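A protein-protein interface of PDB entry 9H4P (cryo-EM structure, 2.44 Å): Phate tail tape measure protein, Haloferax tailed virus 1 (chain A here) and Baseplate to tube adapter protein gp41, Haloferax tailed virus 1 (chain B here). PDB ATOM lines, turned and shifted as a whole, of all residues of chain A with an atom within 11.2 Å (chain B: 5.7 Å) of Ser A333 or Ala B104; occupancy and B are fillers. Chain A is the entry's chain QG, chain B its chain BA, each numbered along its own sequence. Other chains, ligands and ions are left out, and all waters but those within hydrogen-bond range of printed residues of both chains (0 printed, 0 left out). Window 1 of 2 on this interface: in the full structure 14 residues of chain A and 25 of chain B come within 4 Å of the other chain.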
ATOM      1  N   ALA A 308     -21.337 -15.797  10.067  1.00  0.00           N
ATOM      2  CA  ALA A 308     -21.228 -15.699   8.617  1.00  0.00           C
ATOM      3  C   ALA A 308     -22.335 -16.490   7.921  1.00  0.00           C
ATOM      4  O   ALA A 308     -22.920 -16.001   6.960  1.00  0.00           O
ATOM      5  CB  ALA A 308     -19.858 -16.134   8.167  1.00  0.00           C
ATOM      6  N   PHE A 311     -25.635 -14.620   8.274  1.00  0.00           N
ATOM      7  CA  PHE A 311     -25.586 -13.382   7.506  1.00  0.00           C
ATOM      8  C   PHE A 311     -25.821 -13.644   6.016  1.00  0.00           C
ATOM      9  O   PHE A 311     -26.430 -12.814   5.347  1.00  0.00           O
ATOM     10  CB  PHE A 311     -24.293 -12.608   7.788  1.00  0.00           C
ATOM     11  CG  PHE A 311     -24.101 -11.310   7.041  1.00  0.00           C
ATOM     12  CD1 PHE A 311     -25.100 -10.351   7.004  1.00  0.00           C
ATOM     13  CD2 PHE A 311     -22.901 -11.029   6.405  1.00  0.00           C
ATOM     14  CE1 PHE A 311     -24.913  -9.158   6.322  1.00  0.00           C
ATOM     15  CE2 PHE A 311     -22.714  -9.835   5.727  1.00  0.00           C
ATOM     16  CZ  PHE A 311     -23.721  -8.902   5.688  1.00  0.00           C
ATOM     17  N   PHE A 312     -25.360 -14.799   5.507  1.00  0.00           N
ATOM     18  CA  PHE A 312     -25.559 -15.172   4.108  1.00  0.00           C
ATOM     19  C   PHE A 312     -26.945 -15.790   3.895  1.00  0.00           C
ATOM     20  O   PHE A 312     -27.236 -16.262   2.800  1.00  0.00           O
ATOM     21  CB  PHE A 312     -24.416 -16.049   3.571  1.00  0.00           C
ATOM     22  CG  PHE A 312     -23.795 -15.641   2.252  1.00  0.00           C
ATOM     23  CD1 PHE A 312     -24.571 -15.338   1.142  1.00  0.00           C
ATOM     24  CD2 PHE A 312     -22.416 -15.592   2.107  1.00  0.00           C
ATOM     25  CE1 PHE A 312     -23.988 -14.976  -0.063  1.00  0.00           C
ATOM     26  CE2 PHE A 312     -21.833 -15.227   0.903  1.00  0.00           C
ATOM     27  CZ  PHE A 312     -22.620 -14.914  -0.179  1.00  0.00           C
ATOM     28  N   THR A 328     -30.948 -11.114 -10.961  1.00  0.00           N
ATOM     29  CA  THR A 328     -29.838 -10.196 -11.183  1.00  0.00           C
ATOM     30  C   THR A 328     -28.537 -10.950 -10.914  1.00  0.00           C
ATOM     31  O   THR A 328     -28.279 -11.333  -9.772  1.00  0.00           O
ATOM     32  CB  THR A 328     -29.909  -8.966 -10.262  1.00  0.00           C
ATOM     33  OG1 THR A 328     -30.030  -9.391  -8.905  1.00  0.00           O
ATOM     34  CG2 THR A 328     -31.040  -8.017 -10.592  1.00  0.00           C
ATOM     35  N   GLY A 329     -27.722 -11.161 -11.957  1.00  0.00           N
ATOM     36  CA  GLY A 329     -26.517 -11.974 -11.851  1.00  0.00           C
ATOM     37  C   GLY A 329     -25.339 -11.264 -11.180  1.00  0.00           C
ATOM     38  O   GLY A 329     -24.207 -11.398 -11.641  1.00  0.00           O
ATOM     39  N   ARG A 330     -25.610 -10.526 -10.090  1.00  0.00           N
ATOM     40  CA  ARG A 330     -24.598  -9.803  -9.329  1.00  0.00           C
ATOM     41  C   ARG A 330     -24.163 -10.627  -8.123  1.00  0.00           C
ATOM     42  O   ARG A 330     -24.994 -11.185  -7.409  1.00  0.00           O
ATOM     43  CB  ARG A 330     -25.123  -8.449  -8.844  1.00  0.00           C
ATOM     44  CG  ARG A 330     -25.147  -7.382  -9.926  1.00  0.00           C
ATOM     45  CD  ARG A 330     -25.648  -6.059  -9.388  1.00  0.00           C
ATOM     46  NE  ARG A 330     -24.659  -5.325  -8.607  1.00  0.00           N
ATOM     47  CZ  ARG A 330     -24.878  -4.145  -8.037  1.00  0.00           C
ATOM     48  NH1 ARG A 330     -23.918  -3.545  -7.357  1.00  0.00           N
ATOM     49  NH2 ARG A 330     -26.056  -3.560  -8.151  1.00  0.00           N
ATOM     50  N   TYR A 331     -22.848 -10.670  -7.901  1.00  0.00           N
ATOM     51  CA  TYR A 331     -22.279 -11.435  -6.805  1.00  0.00           C
ATOM     52  C   TYR A 331     -22.256 -10.586  -5.534  1.00  0.00           C
ATOM     53  O   TYR A 331     -22.193  -9.357  -5.603  1.00  0.00           O
ATOM     54  CB  TYR A 331     -20.855 -11.891  -7.153  1.00  0.00           C
ATOM     55  CG  TYR A 331     -20.675 -12.852  -8.307  1.00  0.00           C
ATOM     56  CD1 TYR A 331     -21.743 -13.403  -9.010  1.00  0.00           C
ATOM     57  CD2 TYR A 331     -19.397 -13.249  -8.670  1.00  0.00           C
ATOM     58  CE1 TYR A 331     -21.543 -14.294 -10.058  1.00  0.00           C
ATOM     59  CE2 TYR A 331     -19.181 -14.151  -9.699  1.00  0.00           C
ATOM     60  CZ  TYR A 331     -20.256 -14.668 -10.404  1.00  0.00           C
ATOM     61  OH  TYR A 331     -20.054 -15.545 -11.427  1.00  0.00           O
ATOM     62  N   ARG A 332     -22.324 -11.264  -4.380  1.00  0.00           N
ATOM     63  CA  ARG A 332     -21.782 -10.757  -3.125  1.00  0.00           C
ATOM     64  C   ARG A 332     -20.700 -11.718  -2.627  1.00  0.00           C
ATOM     65  O   ARG A 332     -20.777 -12.923  -2.866  1.00  0.00           O
ATOM     66  CB  ARG A 332     -22.863 -10.471  -2.072  1.00  0.00           C
ATOM     67  CG  ARG A 332     -23.666 -11.673  -1.590  1.00  0.00           C
ATOM     68  CD  ARG A 332     -24.227 -11.461  -0.198  1.00  0.00           C
ATOM     69  NE  ARG A 332     -23.285 -11.876   0.834  1.00  0.00           N
ATOM     70  CZ  ARG A 332     -23.312 -11.506   2.110  1.00  0.00           C
ATOM     71  NH1 ARG A 332     -22.393 -11.959   2.945  1.00  0.00           N
ATOM     72  NH2 ARG A 332     -24.238 -10.676   2.552  1.00  0.00           N
ATOM     73  N   SER A 333     -19.684 -11.157  -1.961  1.00  0.00           N
ATOM     74  CA  SER A 333     -18.629 -11.903  -1.291  1.00  0.00           C
ATOM     75  C   SER A 333     -18.429 -11.302   0.098  1.00  0.00           C
ATOM     76  O   SER A 333     -18.631 -10.103   0.262  1.00  0.00           O
ATOM     77  CB  SER A 333     -17.355 -11.900  -2.103  1.00  0.00           C
ATOM     78  OG  SER A 333     -16.968 -10.581  -2.466  1.00  0.00           O
ATOM     79  N   ASP A 334     -18.034 -12.124   1.082  1.00  0.00           N
ATOM     80  CA  ASP A 334     -18.123 -11.762   2.494  1.00  0.00           C
ATOM     81  C   ASP A 334     -17.257 -10.545   2.837  1.00  0.00           C
ATOM     82  O   ASP A 334     -16.180 -10.371   2.263  1.00  0.00           O
ATOM     83  CB  ASP A 334     -17.854 -12.962   3.406  1.00  0.00           C
ATOM     84  CG  ASP A 334     -18.993 -13.965   3.453  1.00  0.00           C
ATOM     85  OD1 ASP A 334     -20.130 -13.582   3.132  1.00  0.00           O
ATOM     86  OD2 ASP A 334     -18.730 -15.118   3.819  1.00  0.00           O
ATOM     87  N   PRO A 335     -17.703  -9.674   3.786  1.00  0.00           N
ATOM     88  CA  PRO A 335     -16.973  -8.454   4.146  1.00  0.00           C
ATOM     89  C   PRO A 335     -15.745  -8.715   5.016  1.00  0.00           C
ATOM     90  O   PRO A 335     -15.551  -9.823   5.513  1.00  0.00           O
ATOM     91  CB  PRO A 335     -18.016  -7.638   4.929  1.00  0.00           C
ATOM     92  CG  PRO A 335     -18.892  -8.683   5.577  1.00  0.00           C
ATOM     93  CD  PRO A 335     -18.951  -9.805   4.562  1.00  0.00           C
ATOM     94  N   SER A 336     -14.944  -7.656   5.195  1.00  0.00           N
ATOM     95  CA  SER A 336     -13.736  -7.634   6.010  1.00  0.00           C
ATOM     96  C   SER A 336     -14.020  -8.077   7.449  1.00  0.00           C
ATOM     97  O   SER A 336     -15.051  -7.710   8.008  1.00  0.00           O
ATOM     98  CB  SER A 336     -13.136  -6.250   5.954  1.00  0.00           C
ATOM     99  OG  SER A 336     -11.914  -6.182   6.661  1.00  0.00           O
ATOM    100  N   ARG A 337     -13.080  -8.830   8.046  1.00  0.00           N
ATOM    101  CA  ARG A 337     -13.233  -9.555   9.307  1.00  0.00           C
ATOM    102  C   ARG A 337     -13.328  -8.632  10.527  1.00  0.00           C
ATOM    103  O   ARG A 337     -13.942  -9.012  11.521  1.00  0.00           O
ATOM    104  CB  ARG A 337     -12.095 -10.566   9.503  1.00  0.00           C
ATOM    105  CG  ARG A 337     -12.007 -11.674   8.459  1.00  0.00           C
ATOM    106  CD  ARG A 337     -13.148 -12.675   8.449  1.00  0.00           C
ATOM    107  NE  ARG A 337     -14.300 -12.133   7.744  1.00  0.00           N
ATOM    108  CZ  ARG A 337     -15.568 -12.458   7.959  1.00  0.00           C
ATOM    109  NH1 ARG A 337     -16.516 -11.878   7.249  1.00  0.00           N
ATOM    110  NH2 ARG A 337     -15.896 -13.347   8.878  1.00  0.00           N
ATOM    111  N   LEU B  55     -17.511 -18.027  -8.464  1.00  0.00           N
ATOM    112  CA  LEU B  55     -17.030 -17.015  -7.535  1.00  0.00           C
ATOM    113  C   LEU B  55     -15.720 -17.500  -6.912  1.00  0.00           C
ATOM    114  O   LEU B  55     -15.650 -18.635  -6.435  1.00  0.00           O
ATOM    115  CB  LEU B  55     -18.102 -16.792  -6.457  1.00  0.00           C
ATOM    116  CG  LEU B  55     -17.726 -15.884  -5.281  1.00  0.00           C
ATOM    117  CD1 LEU B  55     -17.648 -14.422  -5.695  1.00  0.00           C
ATOM    118  CD2 LEU B  55     -18.710 -16.045  -4.132  1.00  0.00           C
ATOM    119  N   THR B  57     -13.154 -15.673  -3.906  1.00  0.00           N
ATOM    120  CA  THR B  57     -12.960 -14.582  -2.960  1.00  0.00           C
ATOM    121  C   THR B  57     -11.659 -14.814  -2.191  1.00  0.00           C
ATOM    122  O   THR B  57     -11.254 -15.960  -1.988  1.00  0.00           O
ATOM    123  CB  THR B  57     -14.139 -14.507  -1.976  1.00  0.00           C
ATOM    124  OG1 THR B  57     -15.347 -14.395  -2.731  1.00  0.00           O
ATOM    125  CG2 THR B  57     -14.055 -13.366  -0.983  1.00  0.00           C
ATOM    126  N   GLN B  59     -10.038 -13.382   1.566  1.00  0.00           N
ATOM    127  CA  GLN B  59      -9.828 -12.567   2.756  1.00  0.00           C
ATOM    128  C   GLN B  59      -8.334 -12.580   3.072  1.00  0.00           C
ATOM    129  O   GLN B  59      -7.751 -13.649   3.262  1.00  0.00           O
ATOM    130  CB  GLN B  59     -10.600 -13.109   3.965  1.00  0.00           C
ATOM    131  CG  GLN B  59     -12.018 -12.562   4.111  1.00  0.00           C
ATOM    132  CD  GLN B  59     -12.999 -13.108   3.099  1.00  0.00           C
ATOM    133  OE1 GLN B  59     -12.973 -14.283   2.737  1.00  0.00           O
ATOM    134  NE2 GLN B  59     -13.887 -12.246   2.632  1.00  0.00           N
ATOM    135  N   ALA B 101     -11.536  -7.176  -7.738  1.00  0.00           N
ATOM    136  CA  ALA B 101     -12.347  -6.055  -7.292  1.00  0.00           C
ATOM    137  C   ALA B 101     -12.398  -6.087  -5.763  1.00  0.00           C
ATOM    138  O   ALA B 101     -12.269  -7.167  -5.179  1.00  0.00           O
ATOM    139  CB  ALA B 101     -13.731  -6.197  -7.887  1.00  0.00           C
ATOM    140  N   PRO B 102     -12.600  -4.936  -5.064  1.00  0.00           N
ATOM    141  CA  PRO B 102     -13.036  -4.961  -3.660  1.00  0.00           C
ATOM    142  C   PRO B 102     -14.300  -5.822  -3.533  1.00  0.00           C
ATOM    143  O   PRO B 102     -15.038  -5.969  -4.510  1.00  0.00           O
ATOM    144  CB  PRO B 102     -13.307  -3.478  -3.342  1.00  0.00           C
ATOM    145  CG  PRO B 102     -12.417  -2.719  -4.312  1.00  0.00           C
ATOM    146  CD  PRO B 102     -12.426  -3.560  -5.574  1.00  0.00           C
ATOM    147  N   ALA B 103     -14.532  -6.398  -2.341  1.00  0.00           N
ATOM    148  CA  ALA B 103     -15.605  -7.362  -2.101  1.00  0.00           C
ATOM    149  C   ALA B 103     -16.922  -6.885  -2.725  1.00  0.00           C
ATOM    150  O   ALA B 103     -17.341  -5.753  -2.484  1.00  0.00           O
ATOM    151  CB  ALA B 103     -15.737  -7.634  -0.620  1.00  0.00           C
ATOM    152  N   ALA B 104     -17.569  -7.775  -3.500  1.00  0.00           N
ATOM    153  CA  ALA B 104     -18.438  -7.439  -4.632  1.00  0.00           C
ATOM    154  C   ALA B 104     -19.595  -6.486  -4.309  1.00  0.00           C
ATOM    155  O   ALA B 104     -19.919  -5.638  -5.142  1.00  0.00           O
ATOM    156  CB  ALA B 104     -18.915  -8.693  -5.333  1.00  0.00           C
ATOM    157  N   GLY B 105     -20.226  -6.629  -3.132  1.00  0.00           N
ATOM    158  CA  GLY B 105     -21.347  -5.774  -2.756  1.00  0.00           C
ATOM    159  C   GLY B 105     -21.214  -5.130  -1.372  1.00  0.00           C
ATOM    160  O   GLY B 105     -22.211  -4.667  -0.816  1.00  0.00           O
ATOM    161  N   GLN B 106     -19.980  -5.064  -0.847  1.00  0.00           N
ATOM    162  CA  GLN B 106     -19.760  -4.820   0.575  1.00  0.00           C
ATOM    163  C   GLN B 106     -19.385  -3.365   0.847  1.00  0.00           C
ATOM    164  O   GLN B 106     -18.611  -2.759   0.099  1.00  0.00           O
ATOM    165  CB  GLN B 106     -18.711  -5.774   1.156  1.00  0.00           C
ATOM    166  CG  GLN B 106     -19.018  -7.250   0.928  1.00  0.00           C
ATOM    167  CD  GLN B 106     -20.452  -7.647   1.190  1.00  0.00           C
ATOM    168  OE1 GLN B 106     -21.175  -8.061   0.287  1.00  0.00           O
ATOM    169  NE2 GLN B 106     -20.880  -7.517   2.435  1.00  0.00           N
ATOM    170  N   LEU B 128     -11.454  -9.353  -1.191  1.00  0.00           N
ATOM    171  CA  LEU B 128     -11.302  -9.133  -2.626  1.00  0.00           C
ATOM    172  C   LEU B 128     -12.034 -10.236  -3.398  1.00  0.00           C
ATOM    173  O   LEU B 128     -12.035 -11.391  -2.972  1.00  0.00           O
ATOM    174  CB  LEU B 128      -9.802  -9.111  -2.967  1.00  0.00           C
ATOM    175  CG  LEU B 128      -8.975  -7.966  -2.365  1.00  0.00           C
ATOM    176  CD1 LEU B 128      -7.481  -8.252  -2.477  1.00  0.00           C
ATOM    177  CD2 LEU B 128      -9.308  -6.622  -3.015  1.00  0.00           C
ATOM    178  N   THR B 129     -12.658  -9.866  -4.527  1.00  0.00           N
ATOM    179  CA  THR B 129     -13.308 -10.814  -5.424  1.00  0.00           C
ATOM    180  C   THR B 129     -12.455 -10.945  -6.686  1.00  0.00           C
ATOM    181  O   THR B 129     -12.067  -9.927  -7.261  1.00  0.00           O
ATOM    182  CB  THR B 129     -14.714 -10.339  -5.832  1.00  0.00           C
ATOM    183  OG1 THR B 129     -15.360  -9.757  -4.698  1.00  0.00           O
ATOM    184  CG2 THR B 129     -15.586 -11.445  -6.391  1.00  0.00           C
ATOM    185  N   ARG B 179     -16.603  -0.413  -2.035  1.00  0.00           N
ATOM    186  CA  ARG B 179     -17.157   0.046  -3.301  1.00  0.00           C
ATOM    187  C   ARG B 179     -18.436  -0.738  -3.614  1.00  0.00           C
ATOM    188  O   ARG B 179     -18.459  -1.515  -4.573  1.00  0.00           O
ATOM    189  CB  ARG B 179     -16.097  -0.086  -4.403  1.00  0.00           C
ATOM    190  CG  ARG B 179     -14.886   0.831  -4.250  1.00  0.00           C
ATOM    191  CD  ARG B 179     -14.036   0.900  -5.510  1.00  0.00           C
ATOM    192  NE  ARG B 179     -14.893   1.192  -6.655  1.00  0.00           N
ATOM    193  CZ  ARG B 179     -15.292   2.403  -7.048  1.00  0.00           C
ATOM    194  NH1 ARG B 179     -16.083   2.517  -8.101  1.00  0.00           N
ATOM    195  NH2 ARG B 179     -14.885   3.493  -6.418  1.00  0.00           N
ATOM    196  N   PRO B 180     -19.541  -0.565  -2.834  1.00  0.00           N
ATOM    197  CA  PRO B 180     -20.759  -1.363  -3.024  1.00  0.00           C
ATOM    198  C   PRO B 180     -21.541  -1.090  -4.313  1.00  0.00           C
ATOM    199  O   PRO B 180     -22.396  -1.894  -4.686  1.00  0.00           O
ATOM    200  CB  PRO B 180     -21.621  -1.042  -1.786  1.00  0.00           C
ATOM    201  CG  PRO B 180     -21.161   0.336  -1.356  1.00  0.00           C
ATOM    202  CD  PRO B 180     -19.689   0.390  -1.717  1.00  0.00           C
ATOM    203  N   ASP B 182     -20.122  -0.711  -7.418  1.00  0.00           N
ATOM    204  CA  ASP B 182     -19.616  -1.465  -8.561  1.00  0.00           C
ATOM    205  C   ASP B 182     -20.484  -2.711  -8.760  1.00  0.00           C
ATOM    206  O   ASP B 182     -21.118  -3.181  -7.813  1.00  0.00           O
ATOM    207  CB  ASP B 182     -18.156  -1.896  -8.370  1.00  0.00           C
ATOM    208  CG  ASP B 182     -17.128  -0.781  -8.469  1.00  0.00           C
ATOM    209  OD1 ASP B 182     -17.442   0.276  -9.060  1.00  0.00           O
ATOM    210  OD2 ASP B 182     -16.008  -0.985  -7.962  1.00  0.00           O
ATOM    211  N   ALA B 183     -20.492  -3.255  -9.988  1.00  0.00           N
ATOM    212  CA  ALA B 183     -21.166  -4.516 -10.269  1.00  0.00           C
ATOM    213  C   ALA B 183     -20.157  -5.569 -10.731  1.00  0.00           C
ATOM    214  O   ALA B 183     -19.427  -5.347 -11.699  1.00  0.00           O
ATOM    215  CB  ALA B 183     -22.271  -4.313 -11.284  1.00  0.00           C
ATOM    216  N   VAL B 184     -20.123  -6.709 -10.023  1.00  0.00           N
ATOM    217  CA  VAL B 184     -19.430  -7.909 -10.477  1.00  0.00           C
ATOM    218  C   VAL B 184     -20.501  -8.870 -11.002  1.00  0.00           C
ATOM    219  O   VAL B 184     -21.397  -9.262 -10.255  1.00  0.00           O
ATOM    220  CB  VAL B 184     -18.560  -8.517  -9.350  1.00  0.00           C
ATOM    221  CG1 VAL B 184     -17.976  -9.876  -9.707  1.00  0.00           C
ATOM    222  CG2 VAL B 184     -17.450  -7.574  -8.895  1.00  0.00           C
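The backbone carbonyl oxygen (O) of Pro B180 sits at hydrogen-bond distance from the guanidinium group (NH1) of Arg A330 (3.5 Å).
The guanidinium group (NH1) of Arg A330 lies within hydrogen-bond range of the backbone carbonyl oxygen (O) of Asp B182 (2.9 Å).
The backbone carbonyl oxygen (O) of Val B184 is in hydrogen-bond range of the backbone NH (N) of Tyr A331, 3.1 Å away.
The side-chain hydroxyl (OG) of Ser A333 lies within hydrogen-bond range of the backbone NH (N) of Ala B104 (3.1 Å).
The backbone carbonyl oxygen (O) of Ser A333 lies close to the side-chain amide oxygen (OE1) of Gln B106, 3.3 Å away.
The side-chain hydroxyl of Thr B129 sits at hydrogen-bond distance from the side-chain hydroxyl of Ser A333 (2.9 Å).
The side-chain amide nitrogen of Gln B59 lies within hydrogen-bond range of the backbone carbonyl oxygen of Asp A334 (3.0 Å).
The guanidinium group of Arg A332 is in salt-bridge range of the side-chain carboxylate of Asp A334, at 2.8 Å.
The backbone carbonyl oxygen (O) of Pro A335 sits at hydrogen-bond distance from the guanidinium group (NH1) of Arg A337.
The backbone carbonyl oxygen (O) of Ala B101 is in hydrogen-bond range of the backbone NH (N) of Thr B129, 2.8 Å away.
The backbone NH (N) of Ala B104 sits at hydrogen-bond distance from the side-chain hydroxyl (OG1) of Thr B129, at 3.2 Å.
The guanidinium group of Arg B179 lies within salt-bridge range of the side-chain carboxylate of Asp B182, at 2.8 Å.
Among the printed residues, merely in contact across the chains: Ser A333 with Thr B57 (3.3 Å), Tyr A331 with Ala B104 (3.4 Å), Arg A330 with Val B184 (3.4 Å), Ser A333 with Ala B103 (3.5 Å), Tyr A331 with Leu B55 (3.6 Å), Pro A335 with Gln B106 (3.7 Å), Arg A330 with Ala B183 (3.7 Å), Arg A332 with Gln B106 (3.8 Å), Gly A329 with Val B184 (3.8 Å), Arg A332 with Leu B55 (3.95 Å) and Asp A334 with Ala B103 (3.9999 Å).
Of the 16 printed residues of chain B, 11 touch a printed residue of chain A.
Hydrophobic or aromatic side chains of chain B that line the printed part of chain A: Leu B55, Ala B103, Ala B104, Ala B183 and Val B184.
Of the 13 printed residues of chain A, 7 touch a printed residue of chain B.
Hydrophobic or aromatic side chains of chain A within 4 Å of the printed part of chain B: Tyr A331 and Pro A335.
Among the printed residues, 18 pairs touch across the chains.
Of the printed residues of chain B, Arg A330 touches Pro B180 (3.5 Å), Asp B182 (2.9 Å), Ala B183 (3.7 Å) and Val B184 (3.4 Å).
Printed residues of chain B within 4 Å of Arg A332: Leu B55 and Gln B106.
Ser A333 touches five residues of chain B.
Printed residues of chain A within 4 Å of Leu B55: Tyr A331 (3.6 Å) and Arg A332 (3.95 Å).
Printed residues of chain A within 4 Å of Gln B59: Asp A334 (3.0 Å).
Ala B101 touches none of the printed residues of chain A.
Pro B102 touches none of the printed residues of chain A.
Printed residues of chain A within 4 Å of Ala B103: Ser A333 (3.5 Å) and Asp A334 (3.9999 Å).
Printed residues of chain A within 4 Å of Ala B104: Tyr A331 and Ser A333.
Of chain A, only Arg A332, Ser A333 and Pro A335 come within 4 Å of Gln B106.
Thr B129 touches just one residue of chain A: Ser A333 (2.9 Å).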
